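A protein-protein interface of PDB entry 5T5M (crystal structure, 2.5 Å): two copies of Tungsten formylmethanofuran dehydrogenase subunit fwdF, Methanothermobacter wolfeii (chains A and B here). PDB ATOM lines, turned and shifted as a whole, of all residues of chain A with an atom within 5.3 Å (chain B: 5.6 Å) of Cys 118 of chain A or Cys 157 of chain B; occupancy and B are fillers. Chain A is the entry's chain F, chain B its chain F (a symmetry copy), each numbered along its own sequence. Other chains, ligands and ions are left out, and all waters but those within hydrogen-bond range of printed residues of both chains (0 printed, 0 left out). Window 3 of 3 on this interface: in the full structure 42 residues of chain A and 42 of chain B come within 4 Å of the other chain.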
ATOM      1  N   ILE A 116      22.930  25.343 -31.106  1.00  0.00           N
ATOM      2  CA  ILE A 116      23.212  26.280 -30.024  1.00  0.00           C
ATOM      3  C   ILE A 116      23.417  25.558 -28.694  1.00  0.00           C
ATOM      4  O   ILE A 116      23.417  26.196 -27.639  1.00  0.00           O
ATOM      5  CB  ILE A 116      22.113  27.356 -29.906  1.00  0.00           C
ATOM      6  CG1 ILE A 116      20.757  26.726 -29.593  1.00  0.00           C
ATOM      7  CG2 ILE A 116      22.037  28.172 -31.191  1.00  0.00           C
ATOM      8  CD1 ILE A 116      19.624  27.719 -29.439  1.00  0.00           C
ATOM      9  N   GLN A 117      23.589  24.237 -28.715  1.00  0.00           N
ATOM     10  CA  GLN A 117      23.984  23.499 -27.517  1.00  0.00           C
ATOM     11  C   GLN A 117      22.913  23.583 -26.431  1.00  0.00           C
ATOM     12  O   GLN A 117      23.217  23.718 -25.243  1.00  0.00           O
ATOM     13  CB  GLN A 117      25.335  24.000 -26.991  1.00  0.00           C
ATOM     14  CG  GLN A 117      26.537  23.613 -27.863  1.00  0.00           C
ATOM     15  CD  GLN A 117      26.693  24.481 -29.106  1.00  0.00           C
ATOM     16  OE1 GLN A 117      26.563  25.704 -29.040  1.00  0.00           O
ATOM     17  NE2 GLN A 117      26.979  23.850 -30.244  1.00  0.00           N
ATOM     18  N   CYS A 118      21.641  23.491 -26.841  1.00  0.00           N
ATOM     19  CA  CYS A 118      20.532  23.576 -25.898  1.00  0.00           C
ATOM     20  C   CYS A 118      20.291  22.267 -25.161  1.00  0.00           C
ATOM     21  O   CYS A 118      19.676  22.280 -24.093  1.00  0.00           O
ATOM     22  CB  CYS A 118      19.253  24.016 -26.625  1.00  0.00           C
ATOM     23  SG  CYS A 118      18.180  22.675 -27.287  1.00  0.00           S
ATOM     24  N   LYS A 119      20.755  21.146 -25.714  1.00  0.00           N
ATOM     25  CA  LYS A 119      20.704  19.811 -25.122  1.00  0.00           C
ATOM     26  C   LYS A 119      19.333  19.157 -25.184  1.00  0.00           C
ATOM     27  O   LYS A 119      19.154  18.080 -24.608  1.00  0.00           O
ATOM     28  CB  LYS A 119      21.183  19.808 -23.667  1.00  0.00           C
ATOM     29  CG  LYS A 119      22.673  20.038 -23.525  1.00  0.00           C
ATOM     30  CD  LYS A 119      23.185  19.504 -22.213  1.00  0.00           C
ATOM     31  CE  LYS A 119      24.693  19.554 -22.158  1.00  0.00           C
ATOM     32  NZ  LYS A 119      25.218  18.756 -21.020  1.00  0.00           N
ATOM     33  N   ALA A 120      18.365  19.749 -25.887  1.00  0.00           N
ATOM     34  CA  ALA A 120      17.047  19.124 -25.983  1.00  0.00           C
ATOM     35  C   ALA A 120      17.125  17.761 -26.673  1.00  0.00           C
ATOM     36  O   ALA A 120      16.509  16.791 -26.220  1.00  0.00           O
ATOM     37  CB  ALA A 120      16.074  20.047 -26.723  1.00  0.00           C
ATOM     38  N   CYS A 121      17.874  17.662 -27.773  1.00  0.00           N
ATOM     39  CA  CYS A 121      17.961  16.382 -28.470  1.00  0.00           C
ATOM     40  C   CYS A 121      18.571  15.307 -27.577  1.00  0.00           C
ATOM     41  O   CYS A 121      18.106  14.163 -27.570  1.00  0.00           O
ATOM     42  CB  CYS A 121      18.784  16.537 -29.739  1.00  0.00           C
ATOM     43  SG  CYS A 121      20.478  16.964 -29.360  1.00  0.00           S
ATOM     44  N   ILE A 132      25.890  15.900 -26.185  1.00  0.00           N
ATOM     45  CA  ILE A 132      26.063  17.336 -26.374  1.00  0.00           C
ATOM     46  C   ILE A 132      26.961  17.855 -25.260  1.00  0.00           C
ATOM     47  O   ILE A 132      26.604  17.778 -24.078  1.00  0.00           O
ATOM     48  CB  ILE A 132      24.724  18.084 -26.381  1.00  0.00           C
ATOM     49  CG1 ILE A 132      23.803  17.517 -27.469  1.00  0.00           C
ATOM     50  CG2 ILE A 132      24.963  19.571 -26.603  1.00  0.00           C
ATOM     51  CD1 ILE A 132      24.302  17.727 -28.898  1.00  0.00           C
ATOM     52  N   ARG A 134      29.006  21.331 -23.811  1.00  0.00           N
ATOM     53  CA  ARG A 134      29.008  22.780 -23.966  1.00  0.00           C
ATOM     54  C   ARG A 134      29.852  23.441 -22.886  1.00  0.00           C
ATOM     55  O   ARG A 134      29.890  22.987 -21.738  1.00  0.00           O
ATOM     56  CB  ARG A 134      27.587  23.353 -23.950  1.00  0.00           C
ATOM     57  CG  ARG A 134      26.902  23.359 -22.606  1.00  0.00           C
ATOM     58  CD  ARG A 134      25.486  23.899 -22.738  1.00  0.00           C
ATOM     59  NE  ARG A 134      24.767  23.843 -21.469  1.00  0.00           N
ATOM     60  CZ  ARG A 134      23.444  23.852 -21.368  1.00  0.00           C
ATOM     61  NH1 ARG A 134      22.866  23.804 -20.171  1.00  0.00           N
ATOM     62  NH2 ARG A 134      22.695  23.897 -22.468  1.00  0.00           N
ATOM     63  N   PRO A 250      14.973  23.379 -31.555  1.00  0.00           N
ATOM     64  CA  PRO A 250      14.389  24.716 -31.722  1.00  0.00           C
ATOM     65  C   PRO A 250      14.954  25.520 -32.878  1.00  0.00           C
ATOM     66  O   PRO A 250      14.379  26.561 -33.216  1.00  0.00           O
ATOM     67  CB  PRO A 250      14.721  25.395 -30.387  1.00  0.00           C
ATOM     68  CG  PRO A 250      16.015  24.745 -29.966  1.00  0.00           C
ATOM     69  CD  PRO A 250      15.895  23.313 -30.405  1.00  0.00           C
ATOM     70  N   CYS B 154      11.297  30.902 -24.238  1.00  0.00           N
ATOM     71  CA  CYS B 154      12.223  29.988 -23.586  1.00  0.00           C
ATOM     72  C   CYS B 154      12.240  28.631 -24.287  1.00  0.00           C
ATOM     73  O   CYS B 154      11.192  28.038 -24.556  1.00  0.00           O
ATOM     74  CB  CYS B 154      11.822  29.843 -22.113  1.00  0.00           C
ATOM     75  SG  CYS B 154      12.649  28.546 -21.116  1.00  0.00           S
ATOM     76  N   ILE B 155      13.447  28.160 -24.594  1.00  0.00           N
ATOM     77  CA  ILE B 155      13.689  26.848 -25.181  1.00  0.00           C
ATOM     78  C   ILE B 155      14.255  25.861 -24.169  1.00  0.00           C
ATOM     79  O   ILE B 155      14.612  24.736 -24.545  1.00  0.00           O
ATOM     80  CB  ILE B 155      14.620  26.953 -26.405  1.00  0.00           C
ATOM     81  CG1 ILE B 155      16.024  27.381 -25.972  1.00  0.00           C
ATOM     82  CG2 ILE B 155      14.051  27.955 -27.393  1.00  0.00           C
ATOM     83  CD1 ILE B 155      17.012  27.555 -27.107  1.00  0.00           C
ATOM     84  N   TYR B 156      14.377  26.253 -22.900  1.00  0.00           N
ATOM     85  CA  TYR B 156      14.670  25.324 -21.811  1.00  0.00           C
ATOM     86  C   TYR B 156      16.073  24.722 -21.915  1.00  0.00           C
ATOM     87  O   TYR B 156      16.316  23.602 -21.452  1.00  0.00           O
ATOM     88  CB  TYR B 156      13.600  24.224 -21.733  1.00  0.00           C
ATOM     89  CG  TYR B 156      12.252  24.799 -21.369  1.00  0.00           C
ATOM     90  CD1 TYR B 156      11.979  25.196 -20.060  1.00  0.00           C
ATOM     91  CD2 TYR B 156      11.263  24.981 -22.330  1.00  0.00           C
ATOM     92  CE1 TYR B 156      10.755  25.738 -19.720  1.00  0.00           C
ATOM     93  CE2 TYR B 156      10.031  25.524 -21.994  1.00  0.00           C
ATOM     94  CZ  TYR B 156       9.785  25.902 -20.689  1.00  0.00           C
ATOM     95  OH  TYR B 156       8.572  26.449 -20.332  1.00  0.00           O
ATOM     96  N   CYS B 157      17.014  25.479 -22.488  1.00  0.00           N
ATOM     97  CA  CYS B 157      18.399  25.033 -22.564  1.00  0.00           C
ATOM     98  C   CYS B 157      19.012  24.830 -21.186  1.00  0.00           C
ATOM     99  O   CYS B 157      19.976  24.073 -21.061  1.00  0.00           O
ATOM    100  CB  CYS B 157      19.234  26.038 -23.365  1.00  0.00           C
ATOM    101  SG  CYS B 157      19.660  27.625 -22.497  1.00  0.00           S
ATOM    102  N   GLY B 158      18.481  25.480 -20.154  1.00  0.00           N
ATOM    103  CA  GLY B 158      18.948  25.251 -18.803  1.00  0.00           C
ATOM    104  C   GLY B 158      20.200  26.004 -18.409  1.00  0.00           C
ATOM    105  O   GLY B 158      20.755  25.722 -17.344  1.00  0.00           O
ATOM    106  N   MET B 159      20.655  26.962 -19.223  1.00  0.00           N
ATOM    107  CA  MET B 159      21.892  27.678 -18.931  1.00  0.00           C
ATOM    108  C   MET B 159      21.711  28.695 -17.808  1.00  0.00           C
ATOM    109  O   MET B 159      22.591  28.836 -16.956  1.00  0.00           O
ATOM    110  CB  MET B 159      22.412  28.356 -20.201  1.00  0.00           C
ATOM    111  CG  MET B 159      22.896  27.352 -21.262  1.00  0.00           C
ATOM    112  SD  MET B 159      23.854  28.049 -22.629  1.00  0.00           S
ATOM    113  CE  MET B 159      22.759  29.336 -23.193  1.00  0.00           C
ATOM    114  N   CYS B 160      20.593  29.423 -17.795  1.00  0.00           N
ATOM    115  CA  CYS B 160      20.296  30.314 -16.676  1.00  0.00           C
ATOM    116  C   CYS B 160      20.292  29.552 -15.357  1.00  0.00           C
ATOM    117  O   CYS B 160      20.864  30.009 -14.361  1.00  0.00           O
ATOM    118  CB  CYS B 160      18.941  30.987 -16.883  1.00  0.00           C
ATOM    119  SG  CYS B 160      17.538  29.835 -16.723  1.00  0.00           S
ATOM    120  N   ILE B 171      13.774  24.804 -13.184  1.00  0.00           N
ATOM    121  CA  ILE B 171      13.150  24.291 -14.398  1.00  0.00           C
ATOM    122  C   ILE B 171      12.580  22.917 -14.086  1.00  0.00           C
ATOM    123  O   ILE B 171      13.232  22.103 -13.424  1.00  0.00           O
ATOM    124  CB  ILE B 171      14.157  24.219 -15.564  1.00  0.00           C
ATOM    125  CG1 ILE B 171      14.626  25.629 -15.943  1.00  0.00           C
ATOM    126  CG2 ILE B 171      13.544  23.515 -16.777  1.00  0.00           C
ATOM    127  CD1 ILE B 171      15.776  25.633 -16.932  1.00  0.00           C
ATOM    128  N   PRO B 205      20.157  32.332 -24.736  1.00  0.00           N
ATOM    129  CA  PRO B 205      20.407  32.346 -26.182  1.00  0.00           C
ATOM    130  C   PRO B 205      19.245  32.848 -27.022  1.00  0.00           C
ATOM    131  O   PRO B 205      19.442  33.084 -28.217  1.00  0.00           O
ATOM    132  CB  PRO B 205      20.700  30.878 -26.486  1.00  0.00           C
ATOM    133  CG  PRO B 205      19.850  30.140 -25.494  1.00  0.00           C
ATOM    134  CD  PRO B 205      19.844  30.980 -24.241  1.00  0.00           C
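The backbone carbonyl oxygen (O) of Cys 157 of chain B is in hydrogen-bond range of the guanidinium group (NH1) of Arg 134 of chain A (3.0 Å).
SG of Cys 157 of chain B sits close to N of Met 159 of chain B (3.5 Å). The backbone carbonyl oxygen (O) of Gln 117 of chain A lies within hydrogen-bond range of the guanidinium group (NH2) of Arg 134 of chain A (2.8 Å). The side-chain sulfur of Cys 118 of chain A lies close to the backbone NH of Ala 120 of chain A (3.2 Å).
Among the printed residues, merely in contact across the chains: Cys 118 of chain A with Cys 157 of chain B (3.4 Å), Ile 116 of chain A with Ile 155 of chain B (3.5 Å), Arg 134 of chain A with Met 159 of chain B (3.5 Å), Arg 134 of chain A with Gly 158 of chain B (3.9 Å) and Pro 250 of chain A with Ile 155 of chain B (3.996 Å).
Of chain B, only Cys 157 comes within 4 Å of Cys 118 of chain A. Cys 157 of chain B touches two residues of chain A. Of the printed residues of chain A, Gly 158 of chain B touches Arg 134. Of the printed residues of chain B, Arg 134 of chain A touches Cys 157 (3.0 Å), Gly 158 (3.9 Å) and Met 159 (3.5 Å). Of the printed residues of chain A, Ile 155 of chain B touches Ile 116 and Pro 250. Printed residues of chain B within 4 Å of Ile 116 of chain A: Ile 155 (3.5 Å). Printed residues of chain A within 4 Å of Met 159 of chain B: Arg 134. Ile 132 of chain A touches none of the printed residues of chain B. The nearest printed residue of chain B that does not touch Ile 116 of chain A is Pro 205 of chain B (4.5 Å).
Printed residues of chain B that touch a printed residue of chain A: Ile 155, Cys 157, Gly 158 and Met 159. Hydrophobic or aromatic side chains of chain B that line the printed part of chain A: Ile 155 and Met 159. Among the printed residues, 6 pairs touch across the chains. Among the printed residues, no Asp or Glu carboxylate lies within 4 Å of a Lys or Arg side-chain nitrogen of the other chain.
No position is printed for both chains.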
